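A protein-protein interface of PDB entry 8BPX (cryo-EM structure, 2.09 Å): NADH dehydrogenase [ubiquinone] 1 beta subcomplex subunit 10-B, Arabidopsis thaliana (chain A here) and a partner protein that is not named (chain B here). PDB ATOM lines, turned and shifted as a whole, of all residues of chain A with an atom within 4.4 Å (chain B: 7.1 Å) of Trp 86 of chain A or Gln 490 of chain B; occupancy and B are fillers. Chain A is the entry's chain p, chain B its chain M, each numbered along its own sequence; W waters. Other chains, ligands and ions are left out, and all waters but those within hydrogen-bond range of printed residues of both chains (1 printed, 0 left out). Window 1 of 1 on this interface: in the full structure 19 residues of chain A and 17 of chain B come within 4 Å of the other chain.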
ATOM      1  N   ARG A  34      -9.814 -14.873  24.566  1.00  0.00           N
ATOM      2  CA  ARG A  34     -10.653 -15.125  23.398  1.00  0.00           C
ATOM      3  C   ARG A  34     -10.650 -16.608  23.031  1.00  0.00           C
ATOM      4  O   ARG A  34     -11.708 -17.206  22.789  1.00  0.00           O
ATOM      5  CB  ARG A  34     -10.190 -14.274  22.215  1.00  0.00           C
ATOM      6  CG  ARG A  34     -11.121 -14.347  21.020  1.00  0.00           C
ATOM      7  CD  ARG A  34     -10.438 -13.910  19.738  1.00  0.00           C
ATOM      8  NE  ARG A  34      -9.529 -14.930  19.237  1.00  0.00           N
ATOM      9  CZ  ARG A  34      -8.305 -14.689  18.786  1.00  0.00           C
ATOM     10  NH1 ARG A  34      -7.815 -13.463  18.744  1.00  0.00           N
ATOM     11  NH2 ARG A  34      -7.556 -15.703  18.371  1.00  0.00           N
ATOM     12  N   ILE A  37     -12.652 -18.617  25.658  1.00  0.00           N
ATOM     13  CA  ILE A  37     -14.092 -18.435  25.495  1.00  0.00           C
ATOM     14  C   ILE A  37     -14.598 -19.242  24.308  1.00  0.00           C
ATOM     15  O   ILE A  37     -15.677 -19.845  24.363  1.00  0.00           O
ATOM     16  CB  ILE A  37     -14.425 -16.938  25.349  1.00  0.00           C
ATOM     17  CG1 ILE A  37     -14.245 -16.214  26.684  1.00  0.00           C
ATOM     18  CG2 ILE A  37     -15.831 -16.742  24.802  1.00  0.00           C
ATOM     19  CD1 ILE A  37     -14.086 -14.724  26.537  1.00  0.00           C
ATOM     20  N   VAL A  38     -13.829 -19.264  23.213  1.00  0.00           N
ATOM     21  CA  VAL A  38     -14.224 -20.063  22.058  1.00  0.00           C
ATOM     22  C   VAL A  38     -14.312 -21.537  22.438  1.00  0.00           C
ATOM     23  O   VAL A  38     -15.280 -22.232  22.092  1.00  0.00           O
ATOM     24  CB  VAL A  38     -13.245 -19.833  20.888  1.00  0.00           C
ATOM     25  CG1 VAL A  38     -13.349 -20.954  19.867  1.00  0.00           C
ATOM     26  CG2 VAL A  38     -13.503 -18.493  20.236  1.00  0.00           C
ATOM     27  N   LYS A  41     -17.432 -22.108  24.618  1.00  0.00           N
ATOM     28  CA  LYS A  41     -18.595 -22.092  23.728  1.00  0.00           C
ATOM     29  C   LYS A  41     -18.754 -23.420  22.964  1.00  0.00           C
ATOM     30  O   LYS A  41     -19.872 -23.872  22.897  1.00  0.00           O
ATOM     31  CB  LYS A  41     -18.650 -20.804  22.887  1.00  0.00           C
ATOM     32  CG  LYS A  41     -18.961 -19.534  23.651  1.00  0.00           C
ATOM     33  CD  LYS A  41     -18.999 -18.315  22.782  1.00  0.00           C
ATOM     34  CE  LYS A  41     -19.392 -17.081  23.557  1.00  0.00           C
ATOM     35  NZ  LYS A  41     -19.969 -16.030  22.694  1.00  0.00           N
ATOM     36  N   TRP A  42     -17.674 -24.018  22.472  1.00  0.00           N
ATOM     37  CA  TRP A  42     -17.733 -25.330  21.809  1.00  0.00           C
ATOM     38  C   TRP A  42     -18.159 -26.445  22.806  1.00  0.00           C
ATOM     39  O   TRP A  42     -18.855 -27.320  22.376  1.00  0.00           O
ATOM     40  CB  TRP A  42     -16.455 -25.670  21.040  1.00  0.00           C
ATOM     41  CG  TRP A  42     -16.460 -25.012  19.699  1.00  0.00           C
ATOM     42  CD1 TRP A  42     -15.803 -23.878  19.346  1.00  0.00           C
ATOM     43  CD2 TRP A  42     -17.206 -25.423  18.546  1.00  0.00           C
ATOM     44  NE1 TRP A  42     -16.052 -23.576  18.046  1.00  0.00           N
ATOM     45  CE2 TRP A  42     -16.918 -24.492  17.527  1.00  0.00           C
ATOM     46  CE3 TRP A  42     -18.077 -26.479  18.272  1.00  0.00           C
ATOM     47  CZ2 TRP A  42     -17.470 -24.588  16.254  1.00  0.00           C
ATOM     48  CZ3 TRP A  42     -18.626 -26.572  17.015  1.00  0.00           C
ATOM     49  CH2 TRP A  42     -18.318 -25.645  16.018  1.00  0.00           C
ATOM     50  N   ILE A  45     -21.893 -26.182  22.917  1.00  0.00           N
ATOM     51  CA  ILE A  45     -22.474 -26.696  21.663  1.00  0.00           C
ATOM     52  C   ILE A  45     -22.484 -28.231  21.730  1.00  0.00           C
ATOM     53  O   ILE A  45     -23.555 -28.782  21.530  1.00  0.00           O
ATOM     54  CB  ILE A  45     -21.822 -26.117  20.386  1.00  0.00           C
ATOM     55  CG1 ILE A  45     -22.037 -24.605  20.268  1.00  0.00           C
ATOM     56  CG2 ILE A  45     -22.260 -26.859  19.133  1.00  0.00           C
ATOM     57  CD1 ILE A  45     -20.824 -23.869  19.755  1.00  0.00           C
ATOM     58  N   VAL A  84     -26.804 -20.618  22.786  1.00  0.00           N
ATOM     59  CA  VAL A  84     -25.790 -21.648  22.478  1.00  0.00           C
ATOM     60  C   VAL A  84     -25.012 -21.066  21.307  1.00  0.00           C
ATOM     61  O   VAL A  84     -25.585 -20.337  20.544  1.00  0.00           O
ATOM     62  CB  VAL A  84     -26.369 -23.059  22.167  1.00  0.00           C
ATOM     63  CG1 VAL A  84     -26.986 -23.179  20.786  1.00  0.00           C
ATOM     64  CG2 VAL A  84     -25.348 -24.149  22.427  1.00  0.00           C
ATOM     65  N   GLY A  85     -23.763 -21.368  21.228  1.00  0.00           N
ATOM     66  CA  GLY A  85     -22.887 -20.857  20.160  1.00  0.00           C
ATOM     67  C   GLY A  85     -23.048 -19.413  19.812  1.00  0.00           C
ATOM     68  O   GLY A  85     -23.234 -18.613  20.682  1.00  0.00           O
ATOM     69  N   TRP A  86     -23.162 -19.156  18.538  1.00  0.00           N
ATOM     70  CA  TRP A  86     -23.170 -17.766  18.071  1.00  0.00           C
ATOM     71  C   TRP A  86     -24.450 -17.501  17.264  1.00  0.00           C
ATOM     72  O   TRP A  86     -24.460 -16.529  16.538  1.00  0.00           O
ATOM     73  CB  TRP A  86     -21.844 -17.566  17.344  1.00  0.00           C
ATOM     74  CG  TRP A  86     -20.575 -17.643  18.138  1.00  0.00           C
ATOM     75  CD1 TRP A  86     -19.908 -16.595  18.689  1.00  0.00           C
ATOM     76  CD2 TRP A  86     -19.761 -18.802  18.387  1.00  0.00           C
ATOM     77  NE1 TRP A  86     -18.756 -17.018  19.287  1.00  0.00           N
ATOM     78  CE2 TRP A  86     -18.634 -18.367  19.119  1.00  0.00           C
ATOM     79  CE3 TRP A  86     -19.882 -20.163  18.104  1.00  0.00           C
ATOM     80  CZ2 TRP A  86     -17.639 -19.239  19.551  1.00  0.00           C
ATOM     81  CZ3 TRP A  86     -18.891 -21.021  18.513  1.00  0.00           C
ATOM     82  CH2 TRP A  86     -17.786 -20.567  19.231  1.00  0.00           C
ATOM     83  N   GLY A  87     -25.566 -18.182  17.628  1.00  0.00           N
ATOM     84  CA  GLY A  87     -26.826 -18.008  16.934  1.00  0.00           C
ATOM     85  C   GLY A  87     -27.634 -16.807  17.390  1.00  0.00           C
ATOM     86  O   GLY A  87     -27.096 -15.706  17.524  1.00  0.00           O
ATOM     87  N   SER B 325     -22.810 -11.723   8.228  1.00  0.00           N
ATOM     88  CA  SER B 325     -23.687 -12.291   9.248  1.00  0.00           C
ATOM     89  C   SER B 325     -22.975 -12.535  10.578  1.00  0.00           C
ATOM     90  O   SER B 325     -23.634 -12.536  11.621  1.00  0.00           O
ATOM     91  CB  SER B 325     -24.311 -13.588   8.740  1.00  0.00           C
ATOM     92  OG  SER B 325     -25.298 -13.300   7.771  1.00  0.00           O
ATOM     93  N   LEU B 326     -21.659 -12.748  10.562  1.00  0.00           N
ATOM     94  CA  LEU B 326     -20.838 -12.844  11.774  1.00  0.00           C
ATOM     95  C   LEU B 326     -21.287 -13.980  12.702  1.00  0.00           C
ATOM     96  O   LEU B 326     -21.434 -13.799  13.910  1.00  0.00           O
ATOM     97  CB  LEU B 326     -20.809 -11.509  12.525  1.00  0.00           C
ATOM     98  CG  LEU B 326     -19.544 -10.650  12.406  1.00  0.00           C
ATOM     99  CD1 LEU B 326     -18.316 -11.403  12.901  1.00  0.00           C
ATOM    100  CD2 LEU B 326     -19.341 -10.157  10.977  1.00  0.00           C
ATOM    101  N   ASN B 327     -21.491 -15.164  12.132  1.00  0.00           N
ATOM    102  CA  ASN B 327     -21.681 -16.379  12.916  1.00  0.00           C
ATOM    103  C   ASN B 327     -21.031 -17.540  12.175  1.00  0.00           C
ATOM    104  O   ASN B 327     -20.544 -17.388  11.054  1.00  0.00           O
ATOM    105  CB  ASN B 327     -23.169 -16.665  13.209  1.00  0.00           C
ATOM    106  CG  ASN B 327     -24.060 -16.465  11.998  1.00  0.00           C
ATOM    107  OD1 ASN B 327     -23.816 -17.025  10.933  1.00  0.00           O
ATOM    108  ND2 ASN B 327     -25.105 -15.673  12.162  1.00  0.00           N
ATOM    109  N   ILE B 328     -21.114 -18.773  12.704  1.00  0.00           N
ATOM    110  CA  ILE B 328     -20.390 -19.964  12.146  1.00  0.00           C
ATOM    111  C   ILE B 328     -20.922 -20.358  10.780  1.00  0.00           C
ATOM    112  O   ILE B 328     -20.118 -20.453   9.903  1.00  0.00           O
ATOM    113  CB  ILE B 328     -20.273 -21.197  13.097  1.00  0.00           C
ATOM    114  CG1 ILE B 328     -20.013 -20.794  14.553  1.00  0.00           C
ATOM    115  CG2 ILE B 328     -19.246 -22.190  12.581  1.00  0.00           C
ATOM    116  CD1 ILE B 328     -18.659 -20.207  14.826  1.00  0.00           C
ATOM    117  N   GLN B 329     -22.221 -20.455  10.669  1.00  0.00           N
ATOM    118  CA  GLN B 329     -22.853 -20.742   9.380  1.00  0.00           C
ATOM    119  C   GLN B 329     -22.462 -19.653   8.362  1.00  0.00           C
ATOM    120  O   GLN B 329     -22.033 -20.037   7.306  1.00  0.00           O
ATOM    121  CB  GLN B 329     -24.347 -21.007   9.513  1.00  0.00           C
ATOM    122  CG  GLN B 329     -24.650 -22.185  10.433  1.00  0.00           C
ATOM    123  CD  GLN B 329     -24.735 -21.857  11.907  1.00  0.00           C
ATOM    124  OE1 GLN B 329     -25.005 -20.737  12.308  1.00  0.00           O
ATOM    125  NE2 GLN B 329     -24.528 -22.858  12.738  1.00  0.00           N
ATOM    126  N   GLN B 409     -30.608 -16.129  10.851  1.00  0.00           N
ATOM    127  CA  GLN B 409     -30.517 -15.944  12.293  1.00  0.00           C
ATOM    128  C   GLN B 409     -30.277 -14.492  12.690  1.00  0.00           C
ATOM    129  O   GLN B 409     -30.599 -14.119  13.820  1.00  0.00           O
ATOM    130  CB  GLN B 409     -29.423 -16.843  12.866  1.00  0.00           C
ATOM    131  CG  GLN B 409     -29.862 -18.288  13.015  1.00  0.00           C
ATOM    132  CD  GLN B 409     -28.700 -19.253  13.089  1.00  0.00           C
ATOM    133  OE1 GLN B 409     -28.405 -19.805  14.147  1.00  0.00           O
ATOM    134  NE2 GLN B 409     -28.037 -19.466  11.964  1.00  0.00           N
ATOM    135  N   ARG B 410     -29.745 -13.665  11.791  1.00  0.00           N
ATOM    136  CA  ARG B 410     -29.530 -12.254  12.089  1.00  0.00           C
ATOM    137  C   ARG B 410     -30.683 -11.384  11.597  1.00  0.00           C
ATOM    138  O   ARG B 410     -31.198 -10.552  12.344  1.00  0.00           O
ATOM    139  CB  ARG B 410     -28.215 -11.767  11.465  1.00  0.00           C
ATOM    140  CG  ARG B 410     -26.978 -12.459  11.981  1.00  0.00           C
ATOM    141  CD  ARG B 410     -26.541 -11.922  13.333  1.00  0.00           C
ATOM    142  NE  ARG B 410     -26.795 -10.495  13.490  1.00  0.00           N
ATOM    143  CZ  ARG B 410     -25.943  -9.536  13.155  1.00  0.00           C
ATOM    144  NH1 ARG B 410     -24.771  -9.812  12.609  1.00  0.00           N
ATOM    145  NH2 ARG B 410     -26.278  -8.269  13.371  1.00  0.00           N
ATOM    146  N   HIS B 482     -13.058 -24.618  11.384  1.00  0.00           N
ATOM    147  CA  HIS B 482     -13.891 -24.211  12.544  1.00  0.00           C
ATOM    148  C   HIS B 482     -13.151 -23.410  13.626  1.00  0.00           C
ATOM    149  O   HIS B 482     -13.724 -22.479  14.048  1.00  0.00           O
ATOM    150  CB  HIS B 482     -14.813 -25.344  13.104  1.00  0.00           C
ATOM    151  CG  HIS B 482     -16.048 -25.415  12.275  1.00  0.00           C
ATOM    152  ND1 HIS B 482     -16.699 -26.575  11.998  1.00  0.00           N
ATOM    153  CD2 HIS B 482     -16.675 -24.464  11.555  1.00  0.00           C
ATOM    154  CE1 HIS B 482     -17.733 -26.336  11.228  1.00  0.00           C
ATOM    155  NE2 HIS B 482     -17.729 -25.056  10.927  1.00  0.00           N
ATOM    156  N   SER B 484     -10.452 -21.449  13.429  1.00  0.00           N
ATOM    157  CA  SER B 484     -10.165 -20.115  12.904  1.00  0.00           C
ATOM    158  C   SER B 484     -11.440 -19.300  12.737  1.00  0.00           C
ATOM    159  O   SER B 484     -11.493 -18.126  13.124  1.00  0.00           O
ATOM    160  CB  SER B 484      -9.425 -20.224  11.571  1.00  0.00           C
ATOM    161  OG  SER B 484      -8.143 -20.790  11.739  1.00  0.00           O
ATOM    162  N   VAL B 485     -12.482 -19.913  12.175  1.00  0.00           N
ATOM    163  CA  VAL B 485     -13.744 -19.211  11.973  1.00  0.00           C
ATOM    164  C   VAL B 485     -14.332 -18.786  13.310  1.00  0.00           C
ATOM    165  O   VAL B 485     -14.824 -17.662  13.464  1.00  0.00           O
ATOM    166  CB  VAL B 485     -14.722 -20.094  11.176  1.00  0.00           C
ATOM    167  CG1 VAL B 485     -16.154 -19.591  11.329  1.00  0.00           C
ATOM    168  CG2 VAL B 485     -14.318 -20.163   9.714  1.00  0.00           C
ATOM    169  N   SER B 486     -14.275 -19.679  14.302  1.00  0.00           N
ATOM    170  CA  SER B 486     -14.813 -19.381  15.623  1.00  0.00           C
ATOM    171  C   SER B 486     -14.079 -18.219  16.265  1.00  0.00           C
ATOM    172  O   SER B 486     -14.701 -17.333  16.856  1.00  0.00           O
ATOM    173  CB  SER B 486     -14.724 -20.619  16.513  1.00  0.00           C
ATOM    174  OG  SER B 486     -15.723 -21.558  16.182  1.00  0.00           O
ATOM    175  N   ASN B 487     -12.752 -18.203  16.165  1.00  0.00           N
ATOM    176  CA  ASN B 487     -12.013 -17.105  16.776  1.00  0.00           C
ATOM    177  C   ASN B 487     -12.252 -15.794  16.035  1.00  0.00           C
ATOM    178  O   ASN B 487     -12.286 -14.732  16.663  1.00  0.00           O
ATOM    179  CB  ASN B 487     -10.530 -17.458  16.855  1.00  0.00           C
ATOM    180  CG  ASN B 487     -10.172 -18.133  18.173  1.00  0.00           C
ATOM    181  OD1 ASN B 487      -9.765 -17.485  19.131  1.00  0.00           O
ATOM    182  ND2 ASN B 487     -10.358 -19.446  18.229  1.00  0.00           N
ATOM    183  N   LEU B 488     -12.450 -15.847  14.714  1.00  0.00           N
ATOM    184  CA  LEU B 488     -12.838 -14.646  13.975  1.00  0.00           C
ATOM    185  C   LEU B 488     -14.189 -14.120  14.439  1.00  0.00           C
ATOM    186  O   LEU B 488     -14.368 -12.909  14.608  1.00  0.00           O
ATOM    187  CB  LEU B 488     -12.867 -14.940  12.475  1.00  0.00           C
ATOM    188  CG  LEU B 488     -13.205 -13.798  11.512  1.00  0.00           C
ATOM    189  CD1 LEU B 488     -12.360 -12.553  11.771  1.00  0.00           C
ATOM    190  CD2 LEU B 488     -13.057 -14.265  10.063  1.00  0.00           C
ATOM    191  N   VAL B 489     -15.151 -15.017  14.648  1.00  0.00           N
ATOM    192  CA  VAL B 489     -16.489 -14.600  15.051  1.00  0.00           C
ATOM    193  C   VAL B 489     -16.461 -13.979  16.443  1.00  0.00           C
ATOM    194  O   VAL B 489     -17.180 -13.014  16.720  1.00  0.00           O
ATOM    195  CB  VAL B 489     -17.455 -15.799  14.972  1.00  0.00           C
ATOM    196  CG1 VAL B 489     -18.636 -15.602  15.874  1.00  0.00           C
ATOM    197  CG2 VAL B 489     -17.917 -16.011  13.552  1.00  0.00           C
ATOM    198  N   GLN B 490     -15.622 -14.504  17.331  1.00  0.00           N
ATOM    199  CA  GLN B 490     -15.611 -14.036  18.709  1.00  0.00           C
ATOM    200  C   GLN B 490     -14.760 -12.786  18.917  1.00  0.00           C
ATOM    201  O   GLN B 490     -14.976 -12.068  19.900  1.00  0.00           O
ATOM    202  CB  GLN B 490     -15.145 -15.165  19.630  1.00  0.00           C
ATOM    203  CG  GLN B 490     -15.067 -14.803  21.099  1.00  0.00           C
ATOM    204  CD  GLN B 490     -16.424 -14.845  21.768  1.00  0.00           C
ATOM    205  OE1 GLN B 490     -17.204 -15.770  21.560  1.00  0.00           O
ATOM    206  NE2 GLN B 490     -16.706 -13.847  22.589  1.00  0.00           N
ATOM    207  N   HIS B 491     -13.844 -12.486  18.002  1.00  0.00           N
ATOM    208  CA  HIS B 491     -12.885 -11.409  18.217  1.00  0.00           C
ATOM    209  C   HIS B 491     -13.587 -10.084  18.489  1.00  0.00           C
ATOM    210  O   HIS B 491     -14.492  -9.678  17.755  1.00  0.00           O
ATOM    211  CB  HIS B 491     -11.964 -11.281  17.004  1.00  0.00           C
ATOM    212  CG  HIS B 491     -10.778 -10.406  17.243  1.00  0.00           C
ATOM    213  ND1 HIS B 491      -9.494 -10.900  17.333  1.00  0.00           N
ATOM    214  CD2 HIS B 491     -10.679  -9.068  17.414  1.00  0.00           C
ATOM    215  CE1 HIS B 491      -8.656  -9.903  17.549  1.00  0.00           C
ATOM    216  NE2 HIS B 491      -9.349  -8.781  17.605  1.00  0.00           N
ATOM    217  N   GLY B 492     -13.163  -9.409  19.554  1.00  0.00           N
ATOM    218  CA  GLY B 492     -13.745  -8.149  19.965  1.00  0.00           C
ATOM    219  C   GLY B 492     -14.740  -8.240  21.103  1.00  0.00           C
ATOM    220  O   GLY B 492     -15.111  -7.203  21.658  1.00  0.00           O
ATOM    221  N   LYS B 493     -15.187  -9.439  21.461  1.00  0.00           N
ATOM    222  CA  LYS B 493     -16.129  -9.644  22.552  1.00  0.00           C
ATOM    223  C   LYS B 493     -15.561 -10.642  23.547  1.00  0.00           C
ATOM    224  O   LYS B 493     -14.729 -11.486  23.199  1.00  0.00           O
ATOM    225  CB  LYS B 493     -17.482 -10.141  22.037  1.00  0.00           C
ATOM    226  CG  LYS B 493     -17.864  -9.581  20.694  1.00  0.00           C
ATOM    227  CD  LYS B 493     -18.574 -10.605  19.855  1.00  0.00           C
ATOM    228  CE  LYS B 493     -18.287 -10.391  18.383  1.00  0.00           C
ATOM    229  NZ  LYS B 493     -16.857 -10.620  18.070  1.00  0.00           N
ATOM    230  N   PHE B 494     -16.015 -10.546  24.793  1.00  0.00           N
ATOM    231  CA  PHE B 494     -15.512 -11.409  25.854  1.00  0.00           C
ATOM    232  C   PHE B 494     -16.646 -11.989  26.682  1.00  0.00           C
ATOM    233  O   PHE B 494     -16.537 -12.134  27.902  1.00  0.00           O
ATOM    234  CB  PHE B 494     -14.512 -10.662  26.728  1.00  0.00           C
ATOM    235  CG  PHE B 494     -13.362 -10.107  25.960  1.00  0.00           C
ATOM    236  CD1 PHE B 494     -12.309 -10.923  25.582  1.00  0.00           C
ATOM    237  CD2 PHE B 494     -13.351  -8.783  25.573  1.00  0.00           C
ATOM    238  CE1 PHE B 494     -11.257 -10.414  24.852  1.00  0.00           C
ATOM    239  CE2 PHE B 494     -12.308  -8.275  24.847  1.00  0.00           C
ATOM    240  CZ  PHE B 494     -11.260  -9.090  24.482  1.00  0.00           C
ATOM    241  N   HIS B 495     -17.744 -12.350  26.031  1.00  0.00           N
ATOM    242  CA  HIS B 495     -18.819 -13.075  26.698  1.00  0.00           C
ATOM    243  C   HIS B 495     -19.492 -14.019  25.711  1.00  0.00           C
ATOM    244  O   HIS B 495     -19.247 -13.943  24.509  1.00  0.00           O
ATOM    245  CB  HIS B 495     -19.839 -12.108  27.313  1.00  0.00           C
ATOM    246  CG  HIS B 495     -20.539 -11.246  26.313  1.00  0.00           C
ATOM    247  ND1 HIS B 495     -21.418 -11.747  25.378  1.00  0.00           N
ATOM    248  CD2 HIS B 495     -20.464  -9.914  26.083  1.00  0.00           C
ATOM    249  CE1 HIS B 495     -21.867 -10.761  24.624  1.00  0.00           C
ATOM    250  NE2 HIS B 495     -21.303  -9.638  25.032  1.00  0.00           N
HETATM  251  O   HOH W   1     -26.467 -15.106  14.830  1.00  0.00           O
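NE1 of Trp 42 of chain A is in hydrogen-bond range of OG of Ser 486 of chain B. The guanidinium group of Arg 34 of chain A is in hydrogen-bond range of the side-chain amide oxygen of Asn 487 of chain B. The side-chain amide oxygen of Gln 490 of chain B lies within hydrogen-bond range of the side-chain amino group of Lys 41 of chain A (3.0 Å). The side-chain amide oxygen of Gln 490 of chain B lies within hydrogen-bond range of the indole nitrogen of Trp 86 of chain A (3.0 Å). ND1 of His 491 of chain B lies within hydrogen-bond range of NH1 of Arg 34 of chain A (3.4 Å). O of His 495 of chain B lies within hydrogen-bond range of NZ of Lys 41 of chain A, at 2.9 Å.
OE1 of Gln 329 of chain B lies within hydrogen-bond range of NE2 of Gln 409 of chain B (3.3 Å). The backbone carbonyl oxygen (O) of His 482 of chain B sits at hydrogen-bond distance from the side-chain hydroxyl (OG) of Ser 486 of chain B, at 3.1 Å. The backbone carbonyl oxygen of Val 489 of chain B is in hydrogen-bond range of the side-chain amino group of Lys 493 of chain B. The side-chain amino group of Lys 493 of chain B lies within hydrogen-bond range of the backbone carbonyl oxygen of Gln 490 of chain B. The side-chain amide nitrogen (NE2) of Gln 490 of chain B is in hydrogen-bond range of the backbone carbonyl oxygen (O) of His 495 of chain B, at 3.2 Å. NZ of Lys 493 of chain B lies within hydrogen-bond range of O of His 491 of chain B, at 2.6 Å.
Arg 34 of chain A touches Gln 490 of chain B (CG to CG, 3.97 Å). CG2 of Ile 37 of chain A touches CD of Gln 490 of chain B, at 3.6 Å. Ile 37 of chain A touches Phe 494 of chain B. Val 38 of chain A touches Ser 486 of chain B (CG1 to CB, 3.6 Å). Val 38 of chain A touches Asn 487 of chain B (CG1 to ND2, 3.7 Å). Gln 490 of chain B touches Val 38 of chain A (CB to CG2, 3.8 Å). Asn 327 of chain B touches Trp 86 of chain A (CB to O, 3.6 Å). Ser 486 of chain B touches Trp 86 of chain A (OG to CH2, 3.8 Å). Trp 86 of chain A touches Val 489 of chain B (CD1 to CG1, 3.2 Å). CA of Gly 87 of chain A touches OE1 of Gln 409 of chain B, at 3.7 Å.
Of the printed residues of chain B, Trp 86 of chain A touches Asn 327, Ile 328, Ser 486, Val 489 and Gln 490. Of the printed residues of chain B, Gly 87 of chain A touches Gln 409 (3.7 Å). Of the printed residues of chain A, Ile 328 of chain B touches Trp 86. Of the printed residues of chain A, Asn 487 of chain B touches Arg 34 and Val 38. Of chain A, only Arg 34 (3.97 Å), Ile 37 (3.6 Å), Val 38 (3.8 Å), Lys 41 (3.0 Å) and Trp 86 (3.0 Å) come within 4 Å of Gln 490 of chain B. Printed residues of chain A within 4 Å of Phe 494 of chain B: Ile 37 (3.7 Å). The nearest residue of chain B that does not touch Trp 86 of chain A is Leu 326 of chain B (4.8 Å). The nearest printed residue of chain A that does not touch Gln 490 of chain B is Gly 85 of chain A (6.7 Å). The nearest printed residue of chain B that does not touch Lys 41 of chain A is Lys 493 of chain B (6.3 Å).
Printed residues of chain B that touch a printed residue of chain A: Asn 327, Ile 328, Gln 409, Ser 486, Asn 487, Val 489, Gln 490, His 491, Phe 494 and His 495. Printed residues of chain A that touch a printed residue of chain B: Arg 34, Ile 37, Val 38, Lys 41, Trp 42, Trp 86 and Gly 87. Hydrophobic or aromatic side chains of chain A that line the printed part of chain B: Ile 37, Val 38, Trp 42 and Trp 86. Among the printed residues, 17 pairs touch across the chains.
Water W1 lies within hydrogen-bond range of O of Gly 87 of chain A (2.8 Å), O of Trp 86 of chain A (3.0 Å) and ND2 of Asn 327 of chain B (3.0 Å).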
